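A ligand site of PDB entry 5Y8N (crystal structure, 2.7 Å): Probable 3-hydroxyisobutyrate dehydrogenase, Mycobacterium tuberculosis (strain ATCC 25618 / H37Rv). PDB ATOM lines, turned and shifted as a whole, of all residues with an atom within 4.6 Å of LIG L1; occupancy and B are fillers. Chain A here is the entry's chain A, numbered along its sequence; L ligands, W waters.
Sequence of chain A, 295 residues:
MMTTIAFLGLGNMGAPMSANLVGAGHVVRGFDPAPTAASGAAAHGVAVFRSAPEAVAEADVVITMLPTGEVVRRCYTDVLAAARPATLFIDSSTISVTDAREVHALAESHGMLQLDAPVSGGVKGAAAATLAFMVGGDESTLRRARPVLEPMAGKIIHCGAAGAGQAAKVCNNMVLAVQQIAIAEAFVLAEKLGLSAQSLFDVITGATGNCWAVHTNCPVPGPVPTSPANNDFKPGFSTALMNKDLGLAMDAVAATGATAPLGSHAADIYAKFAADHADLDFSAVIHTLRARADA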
ATOM      1  N   LEU A   8      19.327   6.599  15.846  1.00  0.00           N
ATOM      2  CA  LEU A   8      19.583   6.740  17.273  1.00  0.00           C
ATOM      3  C   LEU A   8      21.049   7.096  17.492  1.00  0.00           C
ATOM      4  O   LEU A   8      21.943   6.311  17.186  1.00  0.00           O
ATOM      5  CB  LEU A   8      19.210   5.431  17.974  1.00  0.00           C
ATOM      6  CG  LEU A   8      17.796   4.890  17.674  1.00  0.00           C
ATOM      7  CD1 LEU A   8      17.539   3.602  18.431  1.00  0.00           C
ATOM      8  CD2 LEU A   8      16.719   5.904  18.018  1.00  0.00           C
ATOM      9  N   GLY A   9      21.282   8.306  18.020  1.00  0.00           N
ATOM     10  CA  GLY A   9      22.637   8.869  18.129  1.00  0.00           C
ATOM     11  C   GLY A   9      22.880   9.837  16.974  1.00  0.00           C
ATOM     12  O   GLY A   9      23.259   9.423  15.897  1.00  0.00           O
ATOM     13  N   LEU A  10      22.661  11.115  17.238  1.00  0.00           N
ATOM     14  CA  LEU A  10      22.694  12.176  16.247  1.00  0.00           C
ATOM     15  C   LEU A  10      23.825  13.164  16.556  1.00  0.00           C
ATOM     16  O   LEU A  10      23.633  14.385  16.499  1.00  0.00           O
ATOM     17  CB  LEU A  10      21.343  12.908  16.227  1.00  0.00           C
ATOM     18  CG  LEU A  10      20.103  12.047  15.927  1.00  0.00           C
ATOM     19  CD1 LEU A  10      18.825  12.751  16.339  1.00  0.00           C
ATOM     20  CD2 LEU A  10      20.054  11.657  14.463  1.00  0.00           C
ATOM     21  N   GLY A  11      25.004  12.618  16.861  1.00  0.00           N
ATOM     22  CA  GLY A  11      26.165  13.433  17.225  1.00  0.00           C
ATOM     23  C   GLY A  11      26.996  13.809  16.009  1.00  0.00           C
ATOM     24  O   GLY A  11      26.466  13.893  14.896  1.00  0.00           O
ATOM     25  N   ASN A  12      28.302  13.998  16.231  1.00  0.00           N
ATOM     26  CA  ASN A  12      29.225  14.461  15.187  1.00  0.00           C
ATOM     27  C   ASN A  12      29.158  13.642  13.891  1.00  0.00           C
ATOM     28  O   ASN A  12      29.297  14.192  12.793  1.00  0.00           O
ATOM     29  CB  ASN A  12      30.677  14.477  15.718  1.00  0.00           C
ATOM     30  CG  ASN A  12      30.909  15.531  16.795  1.00  0.00           C
ATOM     31  OD1 ASN A  12      30.330  16.604  16.749  1.00  0.00           O
ATOM     32  ND2 ASN A  12      31.758  15.218  17.751  1.00  0.00           N
ATOM     33  N   MET A  13      28.956  12.330  14.028  1.00  0.00           N
ATOM     34  CA  MET A  13      28.780  11.439  12.882  1.00  0.00           C
ATOM     35  C   MET A  13      27.315  11.235  12.527  1.00  0.00           C
ATOM     36  O   MET A  13      26.934  11.318  11.367  1.00  0.00           O
ATOM     37  CB  MET A  13      29.426  10.084  13.170  1.00  0.00           C
ATOM     38  CG  MET A  13      30.920  10.137  13.384  1.00  0.00           C
ATOM     39  SD  MET A  13      31.808  10.560  11.865  1.00  0.00           S
ATOM     40  CE  MET A  13      31.703   9.028  10.974  1.00  0.00           C
ATOM     41  N   GLY A  14      26.497  10.946  13.539  1.00  0.00           N
ATOM     42  CA  GLY A  14      25.073  10.672  13.364  1.00  0.00           C
ATOM     43  C   GLY A  14      24.252  11.769  12.716  1.00  0.00           C
ATOM     44  O   GLY A  14      23.308  11.486  11.972  1.00  0.00           O
ATOM     45  N   PHE A  31      16.391  10.234  17.641  1.00  0.00           N
ATOM     46  CA  PHE A  31      16.489  10.461  19.085  1.00  0.00           C
ATOM     47  C   PHE A  31      17.932  10.637  19.491  1.00  0.00           C
ATOM     48  O   PHE A  31      18.796   9.836  19.133  1.00  0.00           O
ATOM     49  CB  PHE A  31      15.876   9.315  19.911  1.00  0.00           C
ATOM     50  CG  PHE A  31      16.242   9.339  21.369  1.00  0.00           C
ATOM     51  CD1 PHE A  31      15.623  10.229  22.228  1.00  0.00           C
ATOM     52  CD2 PHE A  31      17.251   8.528  21.872  1.00  0.00           C
ATOM     53  CE1 PHE A  31      15.970  10.294  23.588  1.00  0.00           C
ATOM     54  CE2 PHE A  31      17.602   8.593  23.219  1.00  0.00           C
ATOM     55  CZ  PHE A  31      16.964   9.472  24.078  1.00  0.00           C
ATOM     56  N   ASP A  32      18.179  11.693  20.284  1.00  0.00           N
ATOM     57  CA  ASP A  32      19.452  11.880  20.973  1.00  0.00           C
ATOM     58  C   ASP A  32      19.137  12.515  22.325  1.00  0.00           C
ATOM     59  O   ASP A  32      18.313  13.425  22.383  1.00  0.00           O
ATOM     60  CB  ASP A  32      20.365  12.768  20.140  1.00  0.00           C
ATOM     61  CG  ASP A  32      21.818  12.678  20.543  1.00  0.00           C
ATOM     62  OD1 ASP A  32      22.142  12.998  21.702  1.00  0.00           O
ATOM     63  OD2 ASP A  32      22.640  12.288  19.687  1.00  0.00           O
ATOM     64  N   PRO A  33      19.787  12.048  23.412  1.00  0.00           N
ATOM     65  CA  PRO A  33      19.538  12.679  24.722  1.00  0.00           C
ATOM     66  C   PRO A  33      20.126  14.084  24.908  1.00  0.00           C
ATOM     67  O   PRO A  33      19.810  14.725  25.924  1.00  0.00           O
ATOM     68  CB  PRO A  33      20.182  11.694  25.717  1.00  0.00           C
ATOM     69  CG  PRO A  33      21.229  10.991  24.920  1.00  0.00           C
ATOM     70  CD  PRO A  33      20.645  10.862  23.536  1.00  0.00           C
ATOM     71  N   ALA A  34      20.968  14.534  23.984  1.00  0.00           N
ATOM     72  CA  ALA A  34      21.469  15.916  23.951  1.00  0.00           C
ATOM     73  C   ALA A  34      20.532  16.811  23.160  1.00  0.00           C
ATOM     74  O   ALA A  34      20.308  16.534  21.975  1.00  0.00           O
ATOM     75  CB  ALA A  34      22.848  15.965  23.322  1.00  0.00           C
ATOM     76  N   ALA A  37      22.161  18.286  19.975  1.00  0.00           N
ATOM     77  CA  ALA A  37      22.240  17.252  18.949  1.00  0.00           C
ATOM     78  C   ALA A  37      20.881  17.050  18.270  1.00  0.00           C
ATOM     79  O   ALA A  37      20.787  17.009  17.044  1.00  0.00           O
ATOM     80  CB  ALA A  37      22.711  15.923  19.549  1.00  0.00           C
ATOM     81  N   MET A  65      24.260   5.029  15.987  1.00  0.00           N
ATOM     82  CA  MET A  65      25.620   5.588  15.929  1.00  0.00           C
ATOM     83  C   MET A  65      25.945   6.096  17.328  1.00  0.00           C
ATOM     84  O   MET A  65      25.756   7.272  17.644  1.00  0.00           O
ATOM     85  CB  MET A  65      25.689   6.706  14.872  1.00  0.00           C
ATOM     86  CG  MET A  65      27.102   7.144  14.508  1.00  0.00           C
ATOM     87  SD  MET A  65      28.021   5.837  13.679  1.00  0.00           S
ATOM     88  CE  MET A  65      29.439   6.699  13.042  1.00  0.00           C
ATOM     89  N   LEU A  66      26.435   5.177  18.157  1.00  0.00           N
ATOM     90  CA  LEU A  66      26.526   5.354  19.610  1.00  0.00           C
ATOM     91  C   LEU A  66      27.962   5.216  20.126  1.00  0.00           C
ATOM     92  O   LEU A  66      28.794   4.627  19.431  1.00  0.00           O
ATOM     93  CB  LEU A  66      25.594   4.370  20.308  1.00  0.00           C
ATOM     94  CG  LEU A  66      24.105   4.449  19.897  1.00  0.00           C
ATOM     95  CD1 LEU A  66      23.314   3.286  20.451  1.00  0.00           C
ATOM     96  CD2 LEU A  66      23.493   5.776  20.356  1.00  0.00           C
ATOM     97  N   PRO A  67      28.258   5.752  21.324  1.00  0.00           N
ATOM     98  CA  PRO A  67      29.676   5.812  21.759  1.00  0.00           C
ATOM     99  C   PRO A  67      30.336   4.472  22.137  1.00  0.00           C
ATOM    100  O   PRO A  67      31.525   4.309  21.871  1.00  0.00           O
ATOM    101  CB  PRO A  67      29.648   6.749  22.984  1.00  0.00           C
ATOM    102  CG  PRO A  67      28.316   7.417  22.937  1.00  0.00           C
ATOM    103  CD  PRO A  67      27.384   6.417  22.304  1.00  0.00           C
ATOM    104  N   VAL A  71      26.329   0.978  25.649  1.00  0.00           N
ATOM    105  CA  VAL A  71      25.259   1.876  25.233  1.00  0.00           C
ATOM    106  C   VAL A  71      24.432   1.289  24.076  1.00  0.00           C
ATOM    107  O   VAL A  71      23.207   1.460  24.061  1.00  0.00           O
ATOM    108  CB  VAL A  71      25.823   3.273  24.828  1.00  0.00           C
ATOM    109  CG1 VAL A  71      24.748   4.182  24.242  1.00  0.00           C
ATOM    110  CG2 VAL A  71      26.474   3.940  26.032  1.00  0.00           C
ATOM    111  N   CYS A  75      20.561   0.257  24.431  1.00  0.00           N
ATOM    112  CA  CYS A  75      19.649   0.805  23.417  1.00  0.00           C
ATOM    113  C   CYS A  75      18.803  -0.284  22.791  1.00  0.00           C
ATOM    114  O   CYS A  75      17.585  -0.127  22.678  1.00  0.00           O
ATOM    115  CB  CYS A  75      20.439   1.549  22.343  1.00  0.00           C
ATOM    116  SG  CYS A  75      19.391   2.430  21.146  1.00  0.00           S
ATOM    117  N   SER A  92      26.319   1.181  13.165  1.00  0.00           N
ATOM    118  CA  SER A  92      27.514   1.834  12.633  1.00  0.00           C
ATOM    119  C   SER A  92      28.450   2.368  13.731  1.00  0.00           C
ATOM    120  O   SER A  92      29.466   3.007  13.439  1.00  0.00           O
ATOM    121  CB  SER A  92      27.132   2.956  11.660  1.00  0.00           C
ATOM    122  OG  SER A  92      26.568   2.404  10.475  1.00  0.00           O
ATOM    123  N   SER A  93      28.098   2.113  14.996  1.00  0.00           N
ATOM    124  CA  SER A  93      29.009   2.377  16.115  1.00  0.00           C
ATOM    125  C   SER A  93      30.266   1.554  15.955  1.00  0.00           C
ATOM    126  O   SER A  93      30.241   0.484  15.320  1.00  0.00           O
ATOM    127  CB  SER A  93      28.337   1.964  17.440  1.00  0.00           C
ATOM    128  OG  SER A  93      27.057   2.553  17.562  1.00  0.00           O
ATOM    129  N   THR A  94      31.355   2.024  16.539  1.00  0.00           N
ATOM    130  CA  THR A  94      32.568   1.228  16.538  1.00  0.00           C
ATOM    131  C   THR A  94      32.664   0.652  17.929  1.00  0.00           C
ATOM    132  O   THR A  94      32.882   1.357  18.897  1.00  0.00           O
ATOM    133  CB  THR A  94      33.806   2.036  16.123  1.00  0.00           C
ATOM    134  OG1 THR A  94      33.689   2.379  14.749  1.00  0.00           O
ATOM    135  CG2 THR A  94      35.005   1.214  16.214  1.00  0.00           C
ATOM    136  N   VAL A 119      32.154   2.687  10.334  1.00  0.00           N
ATOM    137  CA  VAL A 119      32.592   3.546   9.237  1.00  0.00           C
ATOM    138  C   VAL A 119      34.002   4.083   9.405  1.00  0.00           C
ATOM    139  O   VAL A 119      34.524   4.134  10.515  1.00  0.00           O
ATOM    140  CB  VAL A 119      31.595   4.683   8.985  1.00  0.00           C
ATOM    141  CG1 VAL A 119      30.262   4.117   8.480  1.00  0.00           C
ATOM    142  CG2 VAL A 119      31.374   5.540  10.212  1.00  0.00           C
ATOM    143  N   GLY A 122      35.452   9.836   9.082  1.00  0.00           N
ATOM    144  CA  GLY A 122      35.282  10.949  10.006  1.00  0.00           C
ATOM    145  C   GLY A 122      34.073  11.819   9.699  1.00  0.00           C
ATOM    146  O   GLY A 122      33.178  11.420   8.938  1.00  0.00           O
ATOM    147  N   VAL A 123      34.061  13.002  10.303  1.00  0.00           N
ATOM    148  CA  VAL A 123      32.974  13.976  10.097  1.00  0.00           C
ATOM    149  C   VAL A 123      33.008  14.539   8.659  1.00  0.00           C
ATOM    150  O   VAL A 123      31.967  14.757   8.056  1.00  0.00           O
ATOM    151  CB  VAL A 123      33.048  15.109  11.160  1.00  0.00           C
ATOM    152  CG1 VAL A 123      32.033  16.217  10.870  1.00  0.00           C
ATOM    153  CG2 VAL A 123      32.832  14.546  12.555  1.00  0.00           C
ATOM    154  N   LYS A 169      37.755  -3.321  10.517  1.00  0.00           N
ATOM    155  CA  LYS A 169      38.126  -1.938  10.836  1.00  0.00           C
ATOM    156  C   LYS A 169      39.224  -1.893  11.890  1.00  0.00           C
ATOM    157  O   LYS A 169      40.230  -1.192  11.711  1.00  0.00           O
ATOM    158  CB  LYS A 169      36.927  -1.156  11.339  1.00  0.00           C
ATOM    159  CG  LYS A 169      37.186   0.325  11.534  1.00  0.00           C
ATOM    160  CD  LYS A 169      36.080   1.042  12.277  1.00  0.00           C
ATOM    161  CE  LYS A 169      36.579   2.393  12.769  1.00  0.00           C
ATOM    162  NZ  LYS A 169      35.487   3.372  13.097  1.00  0.00           N
ATOM    163  N   LEU A 241      40.497   9.663  19.031  1.00  0.00           N
ATOM    164  CA  LEU A 241      39.788   8.613  18.302  1.00  0.00           C
ATOM    165  C   LEU A 241      40.685   7.421  17.959  1.00  0.00           C
ATOM    166  O   LEU A 241      40.213   6.276  17.972  1.00  0.00           O
ATOM    167  CB  LEU A 241      39.133   9.171  17.026  1.00  0.00           C
ATOM    168  CG  LEU A 241      37.748   9.767  17.267  1.00  0.00           C
ATOM    169  CD1 LEU A 241      37.418  10.866  16.253  1.00  0.00           C
ATOM    170  CD2 LEU A 241      36.684   8.661  17.239  1.00  0.00           C
ATOM    171  N   LYS A 244      40.930   5.516  21.042  1.00  0.00           N
ATOM    172  CA  LYS A 244      39.670   4.798  21.185  1.00  0.00           C
ATOM    173  C   LYS A 244      39.634   3.499  20.373  1.00  0.00           C
ATOM    174  O   LYS A 244      39.226   2.450  20.875  1.00  0.00           O
ATOM    175  CB  LYS A 244      38.502   5.709  20.783  1.00  0.00           C
ATOM    176  CG  LYS A 244      37.151   5.382  21.408  1.00  0.00           C
ATOM    177  CD  LYS A 244      36.271   4.548  20.484  1.00  0.00           C
ATOM    178  CE  LYS A 244      34.804   4.604  20.944  1.00  0.00           C
ATOM    179  NZ  LYS A 244      33.930   3.767  20.053  1.00  0.00           N
HETATM  180  P1  LIG L   1      29.313  11.674  19.534  1.00  0.00           P
HETATM  181  O1  LIG L   1      29.624  11.548  20.999  1.00  0.00           O
HETATM  182  O2  LIG L   1      29.496  12.994  18.810  1.00  0.00           O
HETATM  183  O3  LIG L   1      27.806  11.215  19.277  1.00  0.00           O
HETATM  184  C1  LIG L   1      27.159  10.125  19.947  1.00  0.00           C
HETATM  185  C2  LIG L   1      25.748  10.560  20.291  1.00  0.00           C
HETATM  186  O4  LIG L   1      24.988   9.477  20.794  1.00  0.00           O
HETATM  187  C3  LIG L   1      25.728  11.660  21.353  1.00  0.00           C
HETATM  188  O5  LIG L   1      25.057  12.837  20.839  1.00  0.00           O
HETATM  189  C4  LIG L   1      24.975  11.063  22.527  1.00  0.00           C
HETATM  190  O6  LIG L   1      24.176  12.028  23.226  1.00  0.00           O
HETATM  191  C5  LIG L   1      24.150   9.986  21.834  1.00  0.00           C
HETATM  192  N1  LIG L   1      23.589   8.905  22.708  1.00  0.00           N
HETATM  193  C6  LIG L   1      24.075   8.425  23.873  1.00  0.00           C
HETATM  194  N2  LIG L   1      23.273   7.440  24.341  1.00  0.00           N
HETATM  195  C7  LIG L   1      22.254   7.278  23.474  1.00  0.00           C
HETATM  196  C8  LIG L   1      21.040   6.416  23.344  1.00  0.00           C
HETATM  197  N3  LIG L   1      20.751   5.477  24.291  1.00  0.00           N
HETATM  198  N4  LIG L   1      20.239   6.580  22.263  1.00  0.00           N
HETATM  199  C9  LIG L   1      20.511   7.497  21.308  1.00  0.00           C
HETATM  200  N5  LIG L   1      21.590   8.310  21.364  1.00  0.00           N
HETATM  201  C10 LIG L   1      22.474   8.245  22.393  1.00  0.00           C
HETATM  202  O7  LIG L   1      30.154  10.542  18.751  1.00  0.00           O
HETATM  203  P2  LIG L   1      30.293  10.438  17.143  1.00  0.00           P
HETATM  204  O8  LIG L   1      28.937  10.684  16.505  1.00  0.00           O
HETATM  205  O9  LIG L   1      31.501  11.242  16.739  1.00  0.00           O
HETATM  206  O10 LIG L   1      30.644   8.879  16.910  1.00  0.00           O
HETATM  207  C11 LIG L   1      29.885   7.814  17.505  1.00  0.00           C
HETATM  208  C12 LIG L   1      30.507   6.455  17.156  1.00  0.00           C
HETATM  209  O11 LIG L   1      31.060   6.493  15.854  1.00  0.00           O
HETATM  210  C13 LIG L   1      31.647   6.043  18.102  1.00  0.00           C
HETATM  211  O12 LIG L   1      31.522   4.661  18.441  1.00  0.00           O
HETATM  212  C14 LIG L   1      32.921   6.342  17.323  1.00  0.00           C
HETATM  213  O13 LIG L   1      34.007   5.466  17.671  1.00  0.00           O
HETATM  214  C15 LIG L   1      32.459   6.157  15.878  1.00  0.00           C
HETATM  215  N6  LIG L   1      33.172   6.921  14.842  1.00  0.00           N
HETATM  216  C16 LIG L   1      33.473   8.222  15.013  1.00  0.00           C
HETATM  217  C17 LIG L   1      34.158   8.967  14.026  1.00  0.00           C
HETATM  218  C18 LIG L   1      34.494  10.425  14.228  1.00  0.00           C
HETATM  219  O14 LIG L   1      35.460  10.857  13.628  1.00  0.00           O
HETATM  220  N7  LIG L   1      33.778  11.221  15.020  1.00  0.00           N
HETATM  221  C19 LIG L   1      34.511   8.304  12.841  1.00  0.00           C
HETATM  222  C20 LIG L   1      34.190   6.958  12.682  1.00  0.00           C
HETATM  223  C21 LIG L   1      33.503   6.288  13.696  1.00  0.00           C
HETATM  224  N1  LG2 L   2      38.390   5.185  11.023  1.00  0.00           N
HETATM  225  C1  LG2 L   2      37.604   6.002  11.963  1.00  0.00           C
HETATM  226  C2  LG2 L   2      37.868   7.406  11.483  1.00  0.00           C
HETATM  227  O1  LG2 L   2      38.314   7.439  10.306  1.00  0.00           O
HETATM  228  C3  LG2 L   2      38.093   5.750  13.387  1.00  0.00           C
HETATM  229  O2  LG2 L   2      37.173   6.163  14.365  1.00  0.00           O
HETATM  230  O3  LG2 L   2      37.693   8.403  12.186  1.00  0.00           O
HETATM  231  O   HOH W   1      25.671  13.181  25.129  1.00  0.00           O
HETATM  232  O   HOH W   2      22.581   5.907  26.742  1.00  0.00           O
HETATM  233  O   HOH W   3      21.538   3.406  25.652  1.00  0.00           O
HETATM  234  O   HOH W   4      28.223  11.518  23.722  1.00  0.00           O
HETATM  235  O   HOH W   5      26.132  15.195  21.070  1.00  0.00           O
HETATM  236  O   HOH W   6      18.206   6.593  25.969  1.00  0.00           O
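The backbone NH (N) of Asn 12 sits at hydrogen-bond distance from an oxygen (O2) of LIG L1. N of Thr 94 lies within hydrogen-bond range of O12 of LIG L1 (3.3 Å). An oxygen (O12) of LIG L1 lies within hydrogen-bond range of the backbone carbonyl oxygen (O) of Pro 67 (3.4 Å). The backbone carbonyl oxygen of Leu 66 sits at hydrogen-bond distance from an oxygen (O12) of LIG L1 (2.9 Å). The side-chain amino group (NZ) of Lys 244 is in hydrogen-bond range of an oxygen (O13) of LIG L1, at 2.9 Å. An oxygen (O8) of LIG L1 sits at hydrogen-bond distance from the backbone NH (N) of Met 13, at 3.0 Å. The backbone NH (N) of Gly 9 sits at hydrogen-bond distance from a nitrogen (N5) of LIG L1, 3.4 Å away. NZ of Lys 169 lies within hydrogen-bond range of O2 of LG2 L2. The side-chain amide nitrogen of Asn 12 is in hydrogen-bond range of an oxygen (O2) of LIG L1. OD1 of Asp 32 lies within hydrogen-bond range of O6 of LIG L1, 2.7 Å away. The side-chain sulfur (SD) of Met 13 sits close to a nitrogen (N7) of LIG L1 (3.8 Å).
The side-chain amino group (NZ) of Lys 169 sits at hydrogen-bond distance from the backbone carbonyl oxygen (O) of Val 119, 2.9 Å away. O of Leu 8 is in hydrogen-bond range of N of Met 65 (2.9 Å). The backbone NH of Leu 66 lies within hydrogen-bond range of the side-chain hydroxyl of Ser 93, 2.8 Å away. SD of Met 13 sits at hydrogen-bond distance from N of Val 123 (3.7 Å). The side-chain amino group (NZ) of Lys 244 sits at hydrogen-bond distance from the backbone carbonyl oxygen (O) of Thr 94, at 2.9 Å. The backbone NH (N) of Gly 9 lies within hydrogen-bond range of the backbone carbonyl oxygen (O) of Phe 31, at 3.1 Å. The side-chain carboxylate (OD2) of Asp 32 is in hydrogen-bond range of the backbone NH (N) of Leu 10 (2.7 Å). The side-chain hydroxyl of Thr 94 sits at hydrogen-bond distance from the side-chain amino group of Lys 169, 2.6 Å away.
SD of Met 65 sits close to O11 of LIG L1. Merely in contact with LIG L1: Leu 8, Gly 11, Gly 14, Phe 31, Pro 33, Val 71, Val 119, Gly 122, Lys 169 and Leu 241. Hydrophobic or aromatic side chains within 4 Å of LIG L1: Met 13, Phe 31, Pro 33, Met 65, Leu 66, Val 71 and Leu 241. Within 4 Å of LIG L1: Leu 8, Gly 9, Gly 11, Asn 12, Met 13, Gly 14, Phe 31, Asp 32, Pro 33, Met 65, Leu 66, Pro 67, Val 71, Thr 94, Val 119, Gly 122, Lys 169, Leu 241 and Lys 244. The nearest printed residue that does not touch LIG L1 is Ala 37 (4.1 Å).
Water W3 bridges a nitrogen (N3) of LIG L1 (2.6 Å) and the backbone carbonyl oxygen (O) of Val 71 (3.0 Å).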
